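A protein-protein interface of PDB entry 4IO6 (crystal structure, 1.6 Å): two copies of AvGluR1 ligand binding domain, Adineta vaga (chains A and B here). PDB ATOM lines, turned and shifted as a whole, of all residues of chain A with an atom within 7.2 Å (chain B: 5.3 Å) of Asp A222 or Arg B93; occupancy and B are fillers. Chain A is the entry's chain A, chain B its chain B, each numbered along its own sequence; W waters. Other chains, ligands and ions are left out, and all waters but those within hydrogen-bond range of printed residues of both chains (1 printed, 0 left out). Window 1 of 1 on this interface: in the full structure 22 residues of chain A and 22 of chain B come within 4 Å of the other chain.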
ATOM      1  N   MET A  52      -8.330 -26.664   5.162  1.00  0.00           N
ATOM      2  CA  MET A  52      -8.126 -25.291   4.698  1.00  0.00           C
ATOM      3  C   MET A  52      -8.167 -25.164   3.183  1.00  0.00           C
ATOM      4  O   MET A  52      -8.443 -24.089   2.650  1.00  0.00           O
ATOM      5  CB  MET A  52      -6.790 -24.749   5.194  1.00  0.00           C
ATOM      6  CG  MET A  52      -6.733 -24.654   6.689  1.00  0.00           C
ATOM      7  SD  MET A  52      -5.120 -24.230   7.313  1.00  0.00           S
ATOM      8  CE  MET A  52      -5.187 -22.532   6.918  1.00  0.00           C
ATOM      9  N   PHE A  98       5.406 -16.592  14.006  1.00  0.00           N
ATOM     10  CA  PHE A  98       5.104 -17.981  14.304  1.00  0.00           C
ATOM     11  C   PHE A  98       3.605 -18.127  14.521  1.00  0.00           C
ATOM     12  O   PHE A  98       2.942 -17.274  15.144  1.00  0.00           O
ATOM     13  CB  PHE A  98       5.843 -18.428  15.546  1.00  0.00           C
ATOM     14  CG  PHE A  98       7.340 -18.577  15.365  1.00  0.00           C
ATOM     15  CD1 PHE A  98       8.179 -17.512  15.646  1.00  0.00           C
ATOM     16  CD2 PHE A  98       7.910 -19.767  14.942  1.00  0.00           C
ATOM     17  CE1 PHE A  98       9.560 -17.642  15.521  1.00  0.00           C
ATOM     18  CE2 PHE A  98       9.298 -19.907  14.836  1.00  0.00           C
ATOM     19  CZ  PHE A  98      10.116 -18.845  15.118  1.00  0.00           C
ATOM     20  N   SER A  99       3.094 -19.231  14.031  1.00  0.00           N
ATOM     21  CA  SER A  99       1.751 -19.618  14.344  1.00  0.00           C
ATOM     22  C   SER A  99       1.587 -19.910  15.818  1.00  0.00           C
ATOM     23  O   SER A  99       2.533 -20.021  16.588  1.00  0.00           O
ATOM     24  CB  SER A  99       1.382 -20.863  13.569  1.00  0.00           C
ATOM     25  OG  SER A  99       1.969 -22.033  14.131  1.00  0.00           O
ATOM     26  N   ASN A 100       0.345 -20.058  16.216  1.00  0.00           N
ATOM     27  CA  ASN A 100       0.010 -20.707  17.452  1.00  0.00           C
ATOM     28  C   ASN A 100       0.845 -21.968  17.625  1.00  0.00           C
ATOM     29  O   ASN A 100       1.068 -22.700  16.673  1.00  0.00           O
ATOM     30  CB  ASN A 100      -1.467 -21.101  17.412  1.00  0.00           C
ATOM     31  CG  ASN A 100      -1.988 -21.442  18.755  1.00  0.00           C
ATOM     32  OD1 ASN A 100      -2.402 -20.559  19.497  1.00  0.00           O
ATOM     33  ND2 ASN A 100      -1.938 -22.721  19.109  1.00  0.00           N
ATOM     34  N   SER A 101       1.272 -22.252  18.838  1.00  0.00           N
ATOM     35  CA  SER A 101       2.070 -23.433  19.133  1.00  0.00           C
ATOM     36  C   SER A 101       1.436 -24.719  18.639  1.00  0.00           C
ATOM     37  O   SER A 101       0.210 -24.946  18.846  1.00  0.00           O
ATOM     38  CB  SER A 101       2.293 -23.528  20.642  1.00  0.00           C
ATOM     39  OG  SER A 101       2.780 -24.810  21.033  1.00  0.00           O
ATOM     40  N   ILE A 209       4.716 -23.032  13.592  1.00  0.00           N
ATOM     41  CA  ILE A 209       4.901 -22.951  12.160  1.00  0.00           C
ATOM     42  C   ILE A 209       5.407 -21.569  11.845  1.00  0.00           C
ATOM     43  O   ILE A 209       4.867 -20.564  12.339  1.00  0.00           O
ATOM     44  CB  ILE A 209       3.559 -23.250  11.433  1.00  0.00           C
ATOM     45  CG1 ILE A 209       3.168 -24.708  11.697  1.00  0.00           C
ATOM     46  CG2 ILE A 209       3.649 -22.935   9.945  1.00  0.00           C
ATOM     47  CD1 ILE A 209       1.792 -25.111  11.091  1.00  0.00           C
ATOM     48  N   THR A 211       5.990 -18.358   9.627  1.00  0.00           N
ATOM     49  CA  THR A 211       5.333 -17.635   8.562  1.00  0.00           C
ATOM     50  C   THR A 211       5.992 -16.276   8.361  1.00  0.00           C
ATOM     51  O   THR A 211       6.789 -15.851   9.198  1.00  0.00           O
ATOM     52  CB  THR A 211       3.820 -17.392   8.868  1.00  0.00           C
ATOM     53  OG1 THR A 211       3.670 -16.312   9.793  1.00  0.00           O
ATOM     54  CG2 THR A 211       3.160 -18.608   9.469  1.00  0.00           C
ATOM     55  N   TRP A 215       1.572 -11.621   8.028  1.00  0.00           N
ATOM     56  CA  TRP A 215       1.104 -12.480   6.945  1.00  0.00           C
ATOM     57  C   TRP A 215      -0.397 -12.343   6.751  1.00  0.00           C
ATOM     58  O   TRP A 215      -1.130 -12.355   7.722  1.00  0.00           O
ATOM     59  CB  TRP A 215       1.394 -13.918   7.332  1.00  0.00           C
ATOM     60  CG  TRP A 215       1.371 -14.922   6.223  1.00  0.00           C
ATOM     61  CD1 TRP A 215       1.780 -14.763   4.932  1.00  0.00           C
ATOM     62  CD2 TRP A 215       0.925 -16.271   6.339  1.00  0.00           C
ATOM     63  NE1 TRP A 215       1.628 -15.945   4.242  1.00  0.00           N
ATOM     64  CE2 TRP A 215       1.117 -16.887   5.090  1.00  0.00           C
ATOM     65  CE3 TRP A 215       0.416 -17.026   7.398  1.00  0.00           C
ATOM     66  CZ2 TRP A 215       0.785 -18.218   4.865  1.00  0.00           C
ATOM     67  CZ3 TRP A 215       0.092 -18.328   7.174  1.00  0.00           C
ATOM     68  CH2 TRP A 215       0.285 -18.918   5.921  1.00  0.00           C
ATOM     69  N   TYR A 217      -2.481 -14.516   5.835  1.00  0.00           N
ATOM     70  CA  TYR A 217      -3.216 -15.753   6.123  1.00  0.00           C
ATOM     71  C   TYR A 217      -3.082 -16.177   7.611  1.00  0.00           C
ATOM     72  O   TYR A 217      -3.435 -17.298   7.984  1.00  0.00           O
ATOM     73  CB  TYR A 217      -2.704 -16.853   5.196  1.00  0.00           C
ATOM     74  CG  TYR A 217      -2.826 -16.535   3.721  1.00  0.00           C
ATOM     75  CD1 TYR A 217      -4.075 -16.521   3.110  1.00  0.00           C
ATOM     76  CD2 TYR A 217      -1.707 -16.260   2.944  1.00  0.00           C
ATOM     77  CE1 TYR A 217      -4.199 -16.246   1.757  1.00  0.00           C
ATOM     78  CE2 TYR A 217      -1.824 -15.980   1.581  1.00  0.00           C
ATOM     79  CZ  TYR A 217      -3.075 -15.971   1.005  1.00  0.00           C
ATOM     80  OH  TYR A 217      -3.224 -15.687  -0.343  1.00  0.00           O
ATOM     81  N   ALA A 218      -2.582 -15.286   8.467  1.00  0.00           N
ATOM     82  CA  ALA A 218      -2.233 -15.661   9.855  1.00  0.00           C
ATOM     83  C   ALA A 218      -3.409 -16.241  10.631  1.00  0.00           C
ATOM     84  O   ALA A 218      -3.284 -17.274  11.302  1.00  0.00           O
ATOM     85  CB  ALA A 218      -1.659 -14.475  10.615  1.00  0.00           C
ATOM     86  N   LYS A 219      -4.536 -15.554  10.569  1.00  0.00           N
ATOM     87  CA  LYS A 219      -5.713 -15.988  11.317  1.00  0.00           C
ATOM     88  C   LYS A 219      -6.215 -17.348  10.832  1.00  0.00           C
ATOM     89  O   LYS A 219      -6.531 -18.218  11.633  1.00  0.00           O
ATOM     90  CB  LYS A 219      -6.829 -14.938  11.222  1.00  0.00           C
ATOM     91  CG  LYS A 219      -8.079 -15.327  11.999  1.00  0.00           C
ATOM     92  CD  LYS A 219      -9.324 -14.547  11.570  1.00  0.00           C
ATOM     93  CE  LYS A 219      -9.848 -14.987  10.200  1.00  0.00           C
ATOM     94  NZ  LYS A 219     -10.420 -16.380  10.176  1.00  0.00           N
ATOM     95  N   ASP A 220      -6.302 -17.548   9.519  1.00  0.00           N
ATOM     96  CA  ASP A 220      -6.798 -18.823   8.976  1.00  0.00           C
ATOM     97  C   ASP A 220      -5.947 -19.972   9.525  1.00  0.00           C
ATOM     98  O   ASP A 220      -6.446 -20.999  10.011  1.00  0.00           O
ATOM     99  CB  ASP A 220      -6.788 -18.782   7.433  1.00  0.00           C
ATOM    100  CG  ASP A 220      -7.640 -19.889   6.770  1.00  0.00           C
ATOM    101  OD1 ASP A 220      -8.640 -20.366   7.358  1.00  0.00           O
ATOM    102  OD2 ASP A 220      -7.327 -20.269   5.601  1.00  0.00           O
ATOM    103  N   LEU A 221      -4.633 -19.803   9.477  1.00  0.00           N
ATOM    104  CA  LEU A 221      -3.763 -20.887   9.944  1.00  0.00           C
ATOM    105  C   LEU A 221      -3.915 -21.116  11.448  1.00  0.00           C
ATOM    106  O   LEU A 221      -4.036 -22.258  11.915  1.00  0.00           O
ATOM    107  CB  LEU A 221      -2.307 -20.604   9.596  1.00  0.00           C
ATOM    108  CG  LEU A 221      -1.297 -21.673  10.036  1.00  0.00           C
ATOM    109  CD1 LEU A 221      -1.602 -23.024   9.423  1.00  0.00           C
ATOM    110  CD2 LEU A 221       0.103 -21.233   9.708  1.00  0.00           C
ATOM    111  N   ASP A 222      -3.898 -20.040  12.224  1.00  0.00           N
ATOM    112  CA  ASP A 222      -3.994 -20.147  13.675  1.00  0.00           C
ATOM    113  C   ASP A 222      -5.305 -20.805  14.124  1.00  0.00           C
ATOM    114  O   ASP A 222      -5.304 -21.672  14.978  1.00  0.00           O
ATOM    115  CB  ASP A 222      -3.854 -18.768  14.343  1.00  0.00           C
ATOM    116  CG  ASP A 222      -2.425 -18.320  14.461  1.00  0.00           C
ATOM    117  OD1 ASP A 222      -1.512 -19.131  14.153  1.00  0.00           O
ATOM    118  OD2 ASP A 222      -2.224 -17.162  14.862  1.00  0.00           O
ATOM    119  N   VAL A 223      -6.433 -20.365  13.565  1.00  0.00           N
ATOM    120  CA  VAL A 223      -7.710 -20.969  13.930  1.00  0.00           C
ATOM    121  C   VAL A 223      -7.721 -22.465  13.651  1.00  0.00           C
ATOM    122  O   VAL A 223      -8.221 -23.254  14.448  1.00  0.00           O
ATOM    123  CB  VAL A 223      -8.853 -20.245  13.204  1.00  0.00           C
ATOM    124  CG1 VAL A 223     -10.146 -21.020  13.323  1.00  0.00           C
ATOM    125  CG2 VAL A 223      -9.003 -18.821  13.765  1.00  0.00           C
ATOM    126  N   ASN A 224      -7.144 -22.862  12.525  1.00  0.00           N
ATOM    127  CA  ASN A 224      -7.129 -24.271  12.176  1.00  0.00           C
ATOM    128  C   ASN A 224      -6.193 -25.095  13.032  1.00  0.00           C
ATOM    129  O   ASN A 224      -6.513 -26.226  13.392  1.00  0.00           O
ATOM    130  CB  ASN A 224      -6.824 -24.439  10.688  1.00  0.00           C
ATOM    131  CG  ASN A 224      -8.074 -24.262   9.828  1.00  0.00           C
ATOM    132  OD1 ASN A 224      -8.857 -25.210   9.665  1.00  0.00           O
ATOM    133  ND2 ASN A 224      -8.297 -23.049   9.323  1.00  0.00           N
ATOM    134  N   ILE A 225      -5.009 -24.559  13.365  1.00  0.00           N
ATOM    135  CA  ILE A 225      -4.155 -25.268  14.321  1.00  0.00           C
ATOM    136  C   ILE A 225      -4.867 -25.479  15.658  1.00  0.00           C
ATOM    137  O   ILE A 225      -4.862 -26.563  16.255  1.00  0.00           O
ATOM    138  CB  ILE A 225      -2.854 -24.496  14.570  1.00  0.00           C
ATOM    139  CG1 ILE A 225      -2.029 -24.513  13.310  1.00  0.00           C
ATOM    140  CG2 ILE A 225      -2.052 -25.105  15.731  1.00  0.00           C
ATOM    141  CD1 ILE A 225      -0.895 -23.519  13.393  1.00  0.00           C
ATOM    142  N   LEU A 226      -5.512 -24.430  16.159  1.00  0.00           N
ATOM    143  CA  LEU A 226      -6.199 -24.522  17.435  1.00  0.00           C
ATOM    144  C   LEU A 226      -7.362 -25.515  17.402  1.00  0.00           C
ATOM    145  O   LEU A 226      -7.623 -26.237  18.361  1.00  0.00           O
ATOM    146  CB  LEU A 226      -6.675 -23.130  17.826  1.00  0.00           C
ATOM    147  CG  LEU A 226      -5.548 -22.209  18.258  1.00  0.00           C
ATOM    148  CD1 LEU A 226      -5.980 -20.761  18.266  1.00  0.00           C
ATOM    149  CD2 LEU A 226      -5.105 -22.623  19.680  1.00  0.00           C
ATOM    150  N   SER A 227      -8.044 -25.561  16.271  1.00  0.00           N
ATOM    151  CA  SER A 227      -9.095 -26.544  16.073  1.00  0.00           C
ATOM    152  C   SER A 227      -8.537 -27.979  16.083  1.00  0.00           C
ATOM    153  O   SER A 227      -9.136 -28.881  16.680  1.00  0.00           O
ATOM    154  CB  SER A 227      -9.811 -26.268  14.756  1.00  0.00           C
ATOM    155  OG  SER A 227     -10.891 -27.196  14.623  1.00  0.00           O
ATOM    156  N   LEU A 228      -7.395 -28.202  15.430  1.00  0.00           N
ATOM    157  CA  LEU A 228      -6.773 -29.528  15.499  1.00  0.00           C
ATOM    158  C   LEU A 228      -6.399 -29.878  16.949  1.00  0.00           C
ATOM    159  O   LEU A 228      -6.462 -31.042  17.367  1.00  0.00           O
ATOM    160  CB  LEU A 228      -5.551 -29.622  14.596  1.00  0.00           C
ATOM    161  CG  LEU A 228      -5.782 -29.531  13.098  1.00  0.00           C
ATOM    162  CD1 LEU A 228      -4.480 -29.656  12.354  1.00  0.00           C
ATOM    163  CD2 LEU A 228      -6.755 -30.597  12.639  1.00  0.00           C
ATOM    164  N   THR B  89      -8.063 -20.092  22.339  1.00  0.00           N
ATOM    165  CA  THR B  89      -8.988 -21.007  21.709  1.00  0.00           C
ATOM    166  C   THR B  89      -9.269 -20.582  20.285  1.00  0.00           C
ATOM    167  O   THR B  89      -9.077 -19.426  19.932  1.00  0.00           O
ATOM    168  CB  THR B  89     -10.338 -21.081  22.469  1.00  0.00           C
ATOM    169  OG1 THR B  89     -11.102 -19.891  22.204  1.00  0.00           O
ATOM    170  CG2 THR B  89     -10.137 -21.249  23.984  1.00  0.00           C
ATOM    171  N   SER B  90      -9.709 -21.538  19.475  1.00  0.00           N
ATOM    172  CA  SER B  90     -10.010 -21.272  18.068  1.00  0.00           C
ATOM    173  C   SER B  90     -11.118 -20.227  17.887  1.00  0.00           C
ATOM    174  O   SER B  90     -11.006 -19.352  17.041  1.00  0.00           O
ATOM    175  CB  SER B  90     -10.389 -22.568  17.345  1.00  0.00           C
ATOM    176  OG  SER B  90     -11.581 -23.161  17.872  1.00  0.00           O
ATOM    177  N   ALA B  91     -12.178 -20.314  18.672  1.00  0.00           N
ATOM    178  CA  ALA B  91     -13.267 -19.345  18.533  1.00  0.00           C
ATOM    179  C   ALA B  91     -12.777 -17.953  18.888  1.00  0.00           C
ATOM    180  O   ALA B  91     -13.141 -16.962  18.235  1.00  0.00           O
ATOM    181  CB  ALA B  91     -14.415 -19.724  19.420  1.00  0.00           C
ATOM    182  N   ARG B  92     -11.953 -17.853  19.924  1.00  0.00           N
ATOM    183  CA  ARG B  92     -11.422 -16.540  20.282  1.00  0.00           C
ATOM    184  C   ARG B  92     -10.479 -15.998  19.216  1.00  0.00           C
ATOM    185  O   ARG B  92     -10.500 -14.814  18.907  1.00  0.00           O
ATOM    186  CB  ARG B  92     -10.713 -16.571  21.641  1.00  0.00           C
ATOM    187  CG  ARG B  92     -11.679 -16.787  22.792  1.00  0.00           C
ATOM    188  CD  ARG B  92     -10.983 -17.171  24.091  1.00  0.00           C
ATOM    189  NE  ARG B  92     -11.968 -17.500  25.132  1.00  0.00           N
ATOM    190  CZ  ARG B  92     -11.651 -17.770  26.390  1.00  0.00           C
ATOM    191  NH1 ARG B  92     -10.387 -17.829  26.768  1.00  0.00           N
ATOM    192  NH2 ARG B  92     -12.612 -18.019  27.277  1.00  0.00           N
ATOM    193  N   ARG B  93      -9.624 -16.865  18.682  1.00  0.00           N
ATOM    194  CA  ARG B  93      -8.680 -16.452  17.652  1.00  0.00           C
ATOM    195  C   ARG B  93      -9.363 -15.939  16.381  1.00  0.00           C
ATOM    196  O   ARG B  93      -8.793 -15.170  15.643  1.00  0.00           O
ATOM    197  CB  ARG B  93      -7.721 -17.602  17.354  1.00  0.00           C
ATOM    198  CG  ARG B  93      -6.629 -17.262  16.323  1.00  0.00           C
ATOM    199  CD  ARG B  93      -5.629 -16.261  16.870  1.00  0.00           C
ATOM    200  NE  ARG B  93      -4.687 -15.834  15.839  1.00  0.00           N
ATOM    201  CZ  ARG B  93      -4.876 -14.810  15.011  1.00  0.00           C
ATOM    202  NH1 ARG B  93      -5.994 -14.079  15.028  1.00  0.00           N
ATOM    203  NH2 ARG B  93      -3.942 -14.525  14.104  1.00  0.00           N
ATOM    204  N   GLU B  94     -10.623 -16.313  16.159  1.00  0.00           N
ATOM    205  CA  GLU B  94     -11.364 -15.750  15.030  1.00  0.00           C
ATOM    206  C   GLU B  94     -11.559 -14.238  15.156  1.00  0.00           C
ATOM    207  O   GLU B  94     -11.692 -13.530  14.141  1.00  0.00           O
ATOM    208  CB  GLU B  94     -12.719 -16.459  14.898  1.00  0.00           C
ATOM    209  CG  GLU B  94     -12.624 -17.830  14.257  1.00  0.00           C
ATOM    210  CD  GLU B  94     -12.558 -17.760  12.742  1.00  0.00           C
ATOM    211  OE1 GLU B  94     -12.670 -16.640  12.183  1.00  0.00           O
ATOM    212  OE2 GLU B  94     -12.429 -18.829  12.111  1.00  0.00           O
ATOM    213  N   ILE B  95     -11.582 -13.722  16.384  1.00  0.00           N
ATOM    214  CA  ILE B  95     -11.942 -12.317  16.597  1.00  0.00           C
ATOM    215  C   ILE B  95     -10.857 -11.431  17.256  1.00  0.00           C
ATOM    216  O   ILE B  95     -10.951 -10.194  17.230  1.00  0.00           O
ATOM    217  CB  ILE B  95     -13.288 -12.229  17.399  1.00  0.00           C
ATOM    218  CG1 ILE B  95     -13.104 -12.769  18.824  1.00  0.00           C
ATOM    219  CG2 ILE B  95     -14.402 -13.016  16.676  1.00  0.00           C
ATOM    220  CD1 ILE B  95     -14.259 -12.370  19.773  1.00  0.00           C
ATOM    221  N   VAL B  96      -9.829 -12.056  17.846  1.00  0.00           N
ATOM    222  CA  VAL B  96      -8.700 -11.357  18.450  1.00  0.00           C
ATOM    223  C   VAL B  96      -7.435 -12.148  18.132  1.00  0.00           C
ATOM    224  O   VAL B  96      -7.500 -13.294  17.721  1.00  0.00           O
ATOM    225  CB  VAL B  96      -8.812 -11.210  19.981  1.00  0.00           C
ATOM    226  CG1 VAL B  96     -10.042 -10.344  20.368  1.00  0.00           C
ATOM    227  CG2 VAL B  96      -8.848 -12.584  20.652  1.00  0.00           C
ATOM    228  N   ALA B  97      -6.287 -11.512  18.287  1.00  0.00           N
ATOM    229  CA  ALA B  97      -5.035 -12.231  18.216  1.00  0.00           C
ATOM    230  C   ALA B  97      -4.493 -12.488  19.622  1.00  0.00           C
ATOM    231  O   ALA B  97      -4.987 -11.921  20.618  1.00  0.00           O
ATOM    232  CB  ALA B  97      -4.035 -11.448  17.379  1.00  0.00           C
ATOM    233  N   PHE B  98      -3.488 -13.368  19.697  1.00  0.00           N
ATOM    234  CA  PHE B  98      -2.840 -13.685  20.953  1.00  0.00           C
ATOM    235  C   PHE B  98      -1.341 -13.586  20.775  1.00  0.00           C
ATOM    236  O   PHE B  98      -0.795 -13.928  19.715  1.00  0.00           O
ATOM    237  CB  PHE B  98      -3.171 -15.125  21.378  1.00  0.00           C
ATOM    238  CG  PHE B  98      -4.578 -15.326  21.847  1.00  0.00           C
ATOM    239  CD1 PHE B  98      -5.566 -15.685  20.971  1.00  0.00           C
ATOM    240  CD2 PHE B  98      -4.897 -15.160  23.184  1.00  0.00           C
ATOM    241  CE1 PHE B  98      -6.872 -15.892  21.430  1.00  0.00           C
ATOM    242  CE2 PHE B  98      -6.182 -15.380  23.653  1.00  0.00           C
ATOM    243  CZ  PHE B  98      -7.173 -15.737  22.763  1.00  0.00           C
ATOM    244  N   LYS B 213      -6.612  -8.077  16.386  1.00  0.00           N
ATOM    245  CA  LYS B 213      -6.084  -8.696  15.167  1.00  0.00           C
ATOM    246  C   LYS B 213      -5.248  -7.689  14.385  1.00  0.00           C
ATOM    247  O   LYS B 213      -5.546  -6.487  14.369  1.00  0.00           O
ATOM    248  CB  LYS B 213      -7.224  -9.266  14.314  1.00  0.00           C
ATOM    249  CG  LYS B 213      -7.898 -10.462  14.984  1.00  0.00           C
ATOM    250  CD  LYS B 213      -8.778 -11.240  14.040  1.00  0.00           C
ATOM    251  CE  LYS B 213      -9.924 -10.389  13.497  1.00  0.00           C
ATOM    252  NZ  LYS B 213     -10.885 -11.230  12.724  1.00  0.00           N
HETATM  253  O   HOH W   1      -0.973 -14.224  14.413  1.00  0.00           O
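The side-chain carboxylate (OD2) of Asp A222 is in salt-bridge range of the guanidinium group (NE) of Arg B93, 3.0 Å away. The side-chain carboxylate (OE1) of Glu B94 lies within salt-bridge range of the side-chain amino group (NZ) of Lys A219, at 3.0 Å.
The guanidinium group (NH1) of Arg B93 lies within hydrogen-bond range of the backbone carbonyl oxygen (O) of Val B96 (3.2 Å). N of Asn A100 is in hydrogen-bond range of OD1 of Asp A222, at 2.9 Å. OG1 of Thr B89 lies within hydrogen-bond range of N of Arg B92 (3.2 Å). O of Glu B94 is in hydrogen-bond range of NZ of Lys B213.
Among the printed residues, merely in contact across the chains: Val A223 with Glu B94 (3.4 Å), Lys A219 with Arg B93 (3.6 Å), Val A223 with Ser B90 (3.7 Å), Leu A226 with Arg B93 (3.7 Å), Leu A226 with Thr B89 (3.8 Å), Leu A226 with Ser B90 (3.8 Å), Val A223 with Arg B93 (3.8 Å), Lys A219 with Lys B213 (3.8 Å), Ala A218 with Arg B93 (3.9 Å) and Ser A227 with Ser B90 (3.95 Å).
Of the printed residues of chain B, Asp A222 touches Arg B93. Of the printed residues of chain A, Arg B93 touches Ala A218, Lys A219, Asp A222, Val A223 and Leu A226. Of the printed residues of chain A, Glu B94 touches Lys A219 (3.0 Å) and Val A223 (3.4 Å). Of the printed residues of chain B, Ser A227 touches Ser B90 (3.95 Å). Of the printed residues of chain B, Val A223 touches Ser B90 (3.7 Å), Arg B93 (3.8 Å) and Glu B94 (3.4 Å). Asn A100 touches none of the printed residues of chain B. Leu A228 touches none of the printed residues of chain B. The nearest printed residue of chain A that does not touch Ser B90 is Asp A222 (5.6 Å).
Of the 20 printed residues of chain A, 6 touch a printed residue of chain B. Hydrophobic or aromatic side chains of chain A that line the printed part of chain B: Val A223 and Leu A226. Along chain A the printed residues that touch a printed residue of chain B span positions 218 to 227.
Position printed for both chains: 98.
Water W1 bridges NH2 of Arg B93 (3.0 Å) and OD2 of Asp A222 (3.2 Å).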
